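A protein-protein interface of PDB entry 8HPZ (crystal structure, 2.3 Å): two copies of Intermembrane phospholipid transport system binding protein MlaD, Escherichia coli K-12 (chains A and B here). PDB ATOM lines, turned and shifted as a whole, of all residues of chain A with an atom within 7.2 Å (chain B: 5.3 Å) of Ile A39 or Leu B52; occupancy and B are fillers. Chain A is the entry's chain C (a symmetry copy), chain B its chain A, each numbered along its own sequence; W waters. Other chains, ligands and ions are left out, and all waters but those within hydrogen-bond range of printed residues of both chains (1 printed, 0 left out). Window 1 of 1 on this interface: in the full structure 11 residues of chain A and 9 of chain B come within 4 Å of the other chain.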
ATOM      1  N   VAL A  37      16.545 -20.312 -18.500  1.00  0.00           N
ATOM      2  CA  VAL A  37      15.439 -21.310 -18.621  1.00  0.00           C
ATOM      3  C   VAL A  37      15.956 -22.376 -19.590  1.00  0.00           C
ATOM      4  O   VAL A  37      16.456 -21.967 -20.604  1.00  0.00           O
ATOM      5  CB  VAL A  37      14.159 -20.655 -19.158  1.00  0.00           C
ATOM      6  CG1 VAL A  37      13.027 -21.637 -19.374  1.00  0.00           C
ATOM      7  CG2 VAL A  37      13.704 -19.505 -18.300  1.00  0.00           C
ATOM      8  N   SER A  38      15.871 -23.675 -19.276  1.00  0.00           N
ATOM      9  CA  SER A  38      16.463 -24.757 -20.103  1.00  0.00           C
ATOM     10  C   SER A  38      15.464 -25.909 -20.318  1.00  0.00           C
ATOM     11  O   SER A  38      14.569 -26.108 -19.490  1.00  0.00           O
ATOM     12  CB  SER A  38      17.757 -25.238 -19.532  1.00  0.00           C
ATOM     13  OG  SER A  38      17.544 -25.918 -18.296  1.00  0.00           O
ATOM     14  N   ILE A  39      15.601 -26.582 -21.453  1.00  0.00           N
ATOM     15  CA  ILE A  39      14.890 -27.830 -21.809  1.00  0.00           C
ATOM     16  C   ILE A  39      16.002 -28.835 -22.098  1.00  0.00           C
ATOM     17  O   ILE A  39      16.906 -28.542 -22.957  1.00  0.00           O
ATOM     18  CB  ILE A  39      13.980 -27.615 -23.047  1.00  0.00           C
ATOM     19  CG1 ILE A  39      12.891 -26.599 -22.754  1.00  0.00           C
ATOM     20  CG2 ILE A  39      13.420 -28.934 -23.556  1.00  0.00           C
ATOM     21  CD1 ILE A  39      12.244 -26.016 -23.985  1.00  0.00           C
ATOM     22  N   GLY A  40      15.934 -29.972 -21.440  1.00  0.00           N
ATOM     23  CA  GLY A  40      16.974 -31.022 -21.505  1.00  0.00           C
ATOM     24  C   GLY A  40      18.370 -30.441 -21.315  1.00  0.00           C
ATOM     25  O   GLY A  40      19.291 -30.956 -21.962  1.00  0.00           O
ATOM     26  N   GLY A  41      18.510 -29.430 -20.456  1.00  0.00           N
ATOM     27  CA  GLY A  41      19.786 -28.743 -20.173  1.00  0.00           C
ATOM     28  C   GLY A  41      20.201 -27.687 -21.193  1.00  0.00           C
ATOM     29  O   GLY A  41      21.219 -27.064 -20.964  1.00  0.00           O
ATOM     30  N   VAL A  42      19.475 -27.478 -22.295  1.00  0.00           N
ATOM     31  CA  VAL A  42      19.867 -26.442 -23.301  1.00  0.00           C
ATOM     32  C   VAL A  42      19.092 -25.155 -23.010  1.00  0.00           C
ATOM     33  O   VAL A  42      17.871 -25.191 -22.755  1.00  0.00           O
ATOM     34  CB  VAL A  42      19.654 -26.933 -24.728  1.00  0.00           C
ATOM     35  CG1 VAL A  42      20.154 -25.894 -25.752  1.00  0.00           C
ATOM     36  CG2 VAL A  42      20.328 -28.295 -24.931  1.00  0.00           C
ATOM     37  N   VAL A  43      19.792 -24.044 -22.931  1.00  0.00           N
ATOM     38  CA  VAL A  43      19.154 -22.745 -22.591  1.00  0.00           C
ATOM     39  C   VAL A  43      18.219 -22.383 -23.740  1.00  0.00           C
ATOM     40  O   VAL A  43      18.658 -22.429 -24.842  1.00  0.00           O
ATOM     41  CB  VAL A  43      20.207 -21.664 -22.354  1.00  0.00           C
ATOM     42  CG1 VAL A  43      19.593 -20.285 -22.208  1.00  0.00           C
ATOM     43  CG2 VAL A  43      21.010 -22.005 -21.138  1.00  0.00           C
ATOM     44  N   VAL A  44      16.977 -22.063 -23.444  1.00  0.00           N
ATOM     45  CA  VAL A  44      15.947 -21.650 -24.427  1.00  0.00           C
ATOM     46  C   VAL A  44      15.441 -20.243 -24.128  1.00  0.00           C
ATOM     47  O   VAL A  44      14.606 -19.748 -24.890  1.00  0.00           O
ATOM     48  CB  VAL A  44      14.776 -22.647 -24.428  1.00  0.00           C
ATOM     49  CG1 VAL A  44      15.243 -23.990 -24.928  1.00  0.00           C
ATOM     50  CG2 VAL A  44      14.119 -22.773 -23.082  1.00  0.00           C
ATOM     51  N   GLY A  45      15.869 -19.638 -23.018  1.00  0.00           N
ATOM     52  CA  GLY A  45      15.221 -18.417 -22.488  1.00  0.00           C
ATOM     53  C   GLY A  45      15.904 -17.921 -21.212  1.00  0.00           C
ATOM     54  O   GLY A  45      16.983 -18.454 -20.821  1.00  0.00           O
ATOM     55  N   ILE A  65      11.214 -16.397 -23.729  1.00  0.00           N
ATOM     56  CA  ILE A  65      11.558 -17.668 -24.409  1.00  0.00           C
ATOM     57  C   ILE A  65      11.831 -17.339 -25.869  1.00  0.00           C
ATOM     58  O   ILE A  65      11.023 -16.571 -26.468  1.00  0.00           O
ATOM     59  CB  ILE A  65      10.425 -18.704 -24.260  1.00  0.00           C
ATOM     60  CG1 ILE A  65      10.016 -18.874 -22.809  1.00  0.00           C
ATOM     61  CG2 ILE A  65      10.862 -20.020 -24.874  1.00  0.00           C
ATOM     62  CD1 ILE A  65      11.124 -19.469 -21.945  1.00  0.00           C
ATOM     63  N   ARG A  68      11.820 -19.471 -31.663  1.00  0.00           N
ATOM     64  CA  ARG A  68      11.941 -20.776 -32.359  1.00  0.00           C
ATOM     65  C   ARG A  68      11.527 -21.965 -31.445  1.00  0.00           C
ATOM     66  O   ARG A  68      11.213 -23.030 -32.027  1.00  0.00           O
ATOM     67  CB  ARG A  68      13.359 -20.941 -32.925  1.00  0.00           C
ATOM     68  CG  ARG A  68      14.437 -21.091 -31.863  1.00  0.00           C
ATOM     69  CD  ARG A  68      15.814 -21.258 -32.431  1.00  0.00           C
ATOM     70  NE  ARG A  68      16.778 -20.637 -31.512  1.00  0.00           N
ATOM     71  CZ  ARG A  68      18.051 -21.009 -31.397  1.00  0.00           C
ATOM     72  NH1 ARG A  68      18.542 -21.997 -32.132  1.00  0.00           N
ATOM     73  NH2 ARG A  68      18.843 -20.390 -30.542  1.00  0.00           N
ATOM     74  N   TYR A  69      11.467 -21.829 -30.109  1.00  0.00           N
ATOM     75  CA  TYR A  69      10.963 -22.912 -29.226  1.00  0.00           C
ATOM     76  C   TYR A  69       9.484 -22.652 -28.912  1.00  0.00           C
ATOM     77  O   TYR A  69       9.123 -22.152 -27.800  1.00  0.00           O
ATOM     78  CB  TYR A  69      11.860 -23.057 -27.996  1.00  0.00           C
ATOM     79  CG  TYR A  69      13.324 -23.137 -28.314  1.00  0.00           C
ATOM     80  CD1 TYR A  69      13.831 -24.182 -29.072  1.00  0.00           C
ATOM     81  CD2 TYR A  69      14.210 -22.194 -27.869  1.00  0.00           C
ATOM     82  CE1 TYR A  69      15.181 -24.305 -29.366  1.00  0.00           C
ATOM     83  CE2 TYR A  69      15.569 -22.250 -28.193  1.00  0.00           C
ATOM     84  CZ  TYR A  69      16.058 -23.337 -28.924  1.00  0.00           C
ATOM     85  OH  TYR A  69      17.383 -23.461 -29.208  1.00  0.00           O
ATOM     86  N   ILE A  72       5.364 -25.643 -27.253  1.00  0.00           N
ATOM     87  CA  ILE A  72       5.391 -26.197 -25.891  1.00  0.00           C
ATOM     88  C   ILE A  72       3.960 -26.321 -25.406  1.00  0.00           C
ATOM     89  O   ILE A  72       3.280 -25.322 -25.267  1.00  0.00           O
ATOM     90  CB  ILE A  72       6.244 -25.344 -24.981  1.00  0.00           C
ATOM     91  CG1 ILE A  72       7.614 -25.082 -25.614  1.00  0.00           C
ATOM     92  CG2 ILE A  72       6.282 -25.983 -23.619  1.00  0.00           C
ATOM     93  CD1 ILE A  72       8.476 -24.219 -24.761  1.00  0.00           C
ATOM     94  N   TYR A  90      18.520 -22.403 -11.812  1.00  0.00           N
ATOM     95  CA  TYR A  90      17.944 -22.273 -13.180  1.00  0.00           C
ATOM     96  C   TYR A  90      16.525 -22.820 -13.182  1.00  0.00           C
ATOM     97  O   TYR A  90      16.106 -23.513 -12.191  1.00  0.00           O
ATOM     98  CB  TYR A  90      18.829 -22.942 -14.235  1.00  0.00           C
ATOM     99  CG  TYR A  90      18.924 -24.450 -14.194  1.00  0.00           C
ATOM    100  CD1 TYR A  90      19.842 -25.120 -13.377  1.00  0.00           C
ATOM    101  CD2 TYR A  90      18.122 -25.225 -15.010  1.00  0.00           C
ATOM    102  CE1 TYR A  90      19.952 -26.505 -13.417  1.00  0.00           C
ATOM    103  CE2 TYR A  90      18.228 -26.609 -15.061  1.00  0.00           C
ATOM    104  CZ  TYR A  90      19.140 -27.256 -14.254  1.00  0.00           C
ATOM    105  OH  TYR A  90      19.210 -28.618 -14.236  1.00  0.00           O
ATOM    106  N   LEU A  91      15.776 -22.484 -14.249  1.00  0.00           N
ATOM    107  CA  LEU A  91      14.423 -23.058 -14.460  1.00  0.00           C
ATOM    108  C   LEU A  91      14.511 -24.176 -15.499  1.00  0.00           C
ATOM    109  O   LEU A  91      14.981 -23.928 -16.571  1.00  0.00           O
ATOM    110  CB  LEU A  91      13.477 -21.950 -14.917  1.00  0.00           C
ATOM    111  CG  LEU A  91      13.098 -20.921 -13.864  1.00  0.00           C
ATOM    112  CD1 LEU A  91      12.264 -19.818 -14.461  1.00  0.00           C
ATOM    113  CD2 LEU A  91      12.313 -21.579 -12.750  1.00  0.00           C
ATOM    114  N   ALA A  92      14.051 -25.371 -15.168  1.00  0.00           N
ATOM    115  CA  ALA A  92      13.951 -26.504 -16.096  1.00  0.00           C
ATOM    116  C   ALA A  92      12.515 -26.525 -16.568  1.00  0.00           C
ATOM    117  O   ALA A  92      11.589 -26.591 -15.735  1.00  0.00           O
ATOM    118  CB  ALA A  92      14.359 -27.810 -15.468  1.00  0.00           C
ATOM    119  N   LEU A  93      12.349 -26.363 -17.858  1.00  0.00           N
ATOM    120  CA  LEU A  93      11.017 -26.486 -18.485  1.00  0.00           C
ATOM    121  C   LEU A  93      10.894 -27.926 -18.962  1.00  0.00           C
ATOM    122  O   LEU A  93      11.758 -28.308 -19.698  1.00  0.00           O
ATOM    123  CB  LEU A  93      10.903 -25.432 -19.588  1.00  0.00           C
ATOM    124  CG  LEU A  93       9.470 -25.145 -20.002  1.00  0.00           C
ATOM    125  CD1 LEU A  93       9.409 -24.011 -20.990  1.00  0.00           C
ATOM    126  CD2 LEU A  93       8.881 -26.358 -20.658  1.00  0.00           C
ATOM    127  N   ASN A  94       9.950 -28.686 -18.398  1.00  0.00           N
ATOM    128  CA  ASN A  94       9.638 -30.105 -18.716  1.00  0.00           C
ATOM    129  C   ASN A  94       8.486 -30.100 -19.738  1.00  0.00           C
ATOM    130  O   ASN A  94       7.372 -29.693 -19.355  1.00  0.00           O
ATOM    131  CB  ASN A  94       9.242 -30.960 -17.497  1.00  0.00           C
ATOM    132  CG  ASN A  94       8.582 -32.279 -17.938  1.00  0.00           C
ATOM    133  OD1 ASN A  94       8.961 -32.912 -18.931  1.00  0.00           O
ATOM    134  ND2 ASN A  94       7.526 -32.705 -17.269  1.00  0.00           N
ATOM    135  N   VAL A  95       8.781 -30.451 -20.993  1.00  0.00           N
ATOM    136  CA  VAL A  95       7.831 -30.380 -22.135  1.00  0.00           C
ATOM    137  C   VAL A  95       6.725 -31.425 -21.921  1.00  0.00           C
ATOM    138  O   VAL A  95       7.048 -32.565 -21.691  1.00  0.00           O
ATOM    139  CB  VAL A  95       8.604 -30.591 -23.443  1.00  0.00           C
ATOM    140  CG1 VAL A  95       7.682 -30.567 -24.652  1.00  0.00           C
ATOM    141  CG2 VAL A  95       9.699 -29.546 -23.615  1.00  0.00           C
ATOM    142  N   ILE B  50      26.269 -28.604 -29.186  1.00  0.00           N
ATOM    143  CA  ILE B  50      24.973 -29.036 -28.598  1.00  0.00           C
ATOM    144  C   ILE B  50      23.855 -28.195 -29.224  1.00  0.00           C
ATOM    145  O   ILE B  50      23.919 -27.008 -29.155  1.00  0.00           O
ATOM    146  CB  ILE B  50      25.043 -28.887 -27.075  1.00  0.00           C
ATOM    147  CG1 ILE B  50      26.238 -29.673 -26.518  1.00  0.00           C
ATOM    148  CG2 ILE B  50      23.736 -29.340 -26.451  1.00  0.00           C
ATOM    149  CD1 ILE B  50      26.474 -29.491 -25.067  1.00  0.00           C
ATOM    150  N   THR B  51      22.846 -28.801 -29.841  1.00  0.00           N
ATOM    151  CA  THR B  51      21.643 -28.057 -30.295  1.00  0.00           C
ATOM    152  C   THR B  51      20.411 -28.799 -29.801  1.00  0.00           C
ATOM    153  O   THR B  51      20.457 -30.012 -29.695  1.00  0.00           O
ATOM    154  CB  THR B  51      21.648 -27.772 -31.802  1.00  0.00           C
ATOM    155  OG1 THR B  51      21.673 -29.015 -32.486  1.00  0.00           O
ATOM    156  CG2 THR B  51      22.832 -26.933 -32.215  1.00  0.00           C
ATOM    157  N   LEU B  52      19.395 -28.051 -29.425  1.00  0.00           N
ATOM    158  CA  LEU B  52      18.078 -28.573 -29.074  1.00  0.00           C
ATOM    159  C   LEU B  52      17.290 -28.600 -30.373  1.00  0.00           C
ATOM    160  O   LEU B  52      17.147 -27.595 -30.974  1.00  0.00           O
ATOM    161  CB  LEU B  52      17.490 -27.646 -28.022  1.00  0.00           C
ATOM    162  CG  LEU B  52      16.136 -28.042 -27.471  1.00  0.00           C
ATOM    163  CD1 LEU B  52      16.200 -29.384 -26.731  1.00  0.00           C
ATOM    164  CD2 LEU B  52      15.599 -26.908 -26.572  1.00  0.00           C
ATOM    165  N   ASP B  53      16.840 -29.761 -30.811  1.00  0.00           N
ATOM    166  CA  ASP B  53      16.012 -29.901 -32.034  1.00  0.00           C
ATOM    167  C   ASP B  53      14.615 -29.371 -31.726  1.00  0.00           C
ATOM    168  O   ASP B  53      13.916 -29.904 -30.871  1.00  0.00           O
ATOM    169  CB  ASP B  53      16.010 -31.367 -32.449  1.00  0.00           C
ATOM    170  CG  ASP B  53      15.102 -31.686 -33.618  1.00  0.00           C
ATOM    171  OD1 ASP B  53      14.308 -30.782 -34.060  1.00  0.00           O
ATOM    172  OD2 ASP B  53      15.184 -32.853 -34.060  1.00  0.00           O
ATOM    173  N   PRO B  54      14.111 -28.338 -32.429  1.00  0.00           N
ATOM    174  CA  PRO B  54      12.787 -27.789 -32.109  1.00  0.00           C
ATOM    175  C   PRO B  54      11.632 -28.764 -32.416  1.00  0.00           C
ATOM    176  O   PRO B  54      10.568 -28.574 -31.886  1.00  0.00           O
ATOM    177  CB  PRO B  54      12.713 -26.488 -32.931  1.00  0.00           C
ATOM    178  CG  PRO B  54      14.165 -26.233 -33.411  1.00  0.00           C
ATOM    179  CD  PRO B  54      14.757 -27.629 -33.551  1.00  0.00           C
ATOM    180  N   TYR B  57      12.388 -31.551 -29.164  1.00  0.00           N
ATOM    181  CA  TYR B  57      12.820 -30.914 -27.881  1.00  0.00           C
ATOM    182  C   TYR B  57      13.770 -31.830 -27.117  1.00  0.00           C
ATOM    183  O   TYR B  57      13.766 -31.822 -25.895  1.00  0.00           O
ATOM    184  CB  TYR B  57      11.610 -30.501 -27.031  1.00  0.00           C
ATOM    185  CG  TYR B  57      10.994 -29.202 -27.501  1.00  0.00           C
ATOM    186  CD1 TYR B  57      11.703 -28.016 -27.413  1.00  0.00           C
ATOM    187  CD2 TYR B  57       9.740 -29.149 -28.057  1.00  0.00           C
ATOM    188  CE1 TYR B  57      11.170 -26.815 -27.866  1.00  0.00           C
ATOM    189  CE2 TYR B  57       9.200 -27.959 -28.510  1.00  0.00           C
ATOM    190  CZ  TYR B  57       9.914 -26.787 -28.425  1.00  0.00           C
ATOM    191  OH  TYR B  57       9.371 -25.632 -28.892  1.00  0.00           O
ATOM    192  N   LEU B  58      14.540 -32.626 -27.847  1.00  0.00           N
ATOM    193  CA  LEU B  58      15.612 -33.490 -27.337  1.00  0.00           C
ATOM    194  C   LEU B  58      16.942 -32.891 -27.782  1.00  0.00           C
ATOM    195  O   LEU B  58      17.084 -32.462 -28.923  1.00  0.00           O
ATOM    196  CB  LEU B  58      15.421 -34.903 -27.896  1.00  0.00           C
ATOM    197  CG  LEU B  58      14.178 -35.692 -27.434  1.00  0.00           C
ATOM    198  CD1 LEU B  58      14.265 -37.144 -27.899  1.00  0.00           C
ATOM    199  CD2 LEU B  58      14.014 -35.680 -25.913  1.00  0.00           C
ATOM    200  N   PRO B  59      17.908 -32.699 -26.862  1.00  0.00           N
ATOM    201  CA  PRO B  59      19.257 -32.297 -27.206  1.00  0.00           C
ATOM    202  C   PRO B  59      20.027 -33.279 -28.101  1.00  0.00           C
ATOM    203  O   PRO B  59      20.094 -34.401 -27.835  1.00  0.00           O
ATOM    204  CB  PRO B  59      20.026 -32.224 -25.888  1.00  0.00           C
ATOM    205  CG  PRO B  59      19.005 -32.362 -24.789  1.00  0.00           C
ATOM    206  CD  PRO B  59      17.690 -32.726 -25.421  1.00  0.00           C
ATOM    207  N   ARG B  60      20.646 -32.735 -29.134  1.00  0.00           N
ATOM    208  CA  ARG B  60      21.549 -33.463 -30.032  1.00  0.00           C
ATOM    209  C   ARG B  60      22.975 -32.950 -29.808  1.00  0.00           C
ATOM    210  O   ARG B  60      23.201 -31.738 -29.706  1.00  0.00           O
ATOM    211  CB  ARG B  60      21.128 -33.324 -31.490  1.00  0.00           C
ATOM    212  CG  ARG B  60      21.786 -34.354 -32.394  1.00  0.00           C
ATOM    213  CD  ARG B  60      20.986 -34.285 -33.654  1.00  0.00           C
ATOM    214  NE  ARG B  60      21.815 -33.991 -34.797  1.00  0.00           N
ATOM    215  CZ  ARG B  60      22.185 -34.894 -35.685  1.00  0.00           C
ATOM    216  NH1 ARG B  60      21.847 -36.164 -35.518  1.00  0.00           N
ATOM    217  NH2 ARG B  60      22.910 -34.533 -36.726  1.00  0.00           N
HETATM  218  O   HOH W   1      17.346 -25.019 -32.611  1.00  0.00           O
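Water W1 lies within hydrogen-bond range of O of Leu B52 (3.1 Å) and NH1 of Arg A68 (3.3 Å).
O of Ile A39 touches CD1 of Leu B52 (3.9 Å). Tyr B57 touches Ile A39 (O to CG2, 3.7 Å). Pro B59 touches Gly A40. Val A42 touches Ile B50. CB of Leu B52 touches CG1 of Val A42 (3.9 Å). Val A44 touches Leu B52 (CG1 to CD2, 3.4 Å). Arg A68 touches Pro B54 (O to CB, 3.9 Å). Tyr A69 touches Leu B52 (CE1 to CD2, 3.8 Å). Tyr B57 touches Tyr A69. OH of Tyr B57 touches CG1 of Ile A72, at 3.8 Å.
Of the 9 printed residues of chain B, 5 touch a printed residue of chain A. Printed residues of chain A that touch a printed residue of chain B: Ile A39, Gly A40, Val A42, Val A44, Arg A68, Tyr A69 and Ile A72. Among the printed residues, 10 pairs touch across the chains.
N of Val A44 is in hydrogen-bond range of O of Val A37 (2.9 Å). The guanidinium group (NH1) of Arg A68 lies close to the side-chain hydroxyl (OH) of Tyr A69 (3.5 Å).
No position is printed for both chains. Of the 10 pairs that touch across the chains among the printed residues, none has its exchanged pair printed and touching as well.
Of chain B, only Leu B52 and Tyr B57 come within 4 Å of Ile A39. Of the printed residues of chain A, Leu B52 touches Ile A39 (3.9 Å), Val A42 (3.9 Å), Val A44 (3.4 Å) and Tyr A69 (3.8 Å). Of the printed residues of chain A, Pro B59 touches Gly A40. Of the printed residues of chain B, Val A44 touches Leu B52 (3.4 Å). Printed residues of chain B within 4 Å of Tyr A69: Leu B52 (3.8 Å) and Tyr B57 (3.0 Å). Printed residues of chain B within 4 Å of Ile A72: Tyr B57. Of the printed residues of chain A, Ile B50 touches Val A42. Tyr A90 touches none of the printed residues of chain B. Arg B60 touches none of the printed residues of chain A. The nearest residue of chain B that does not touch Ile A39 is Pro B59 (4.7 Å).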
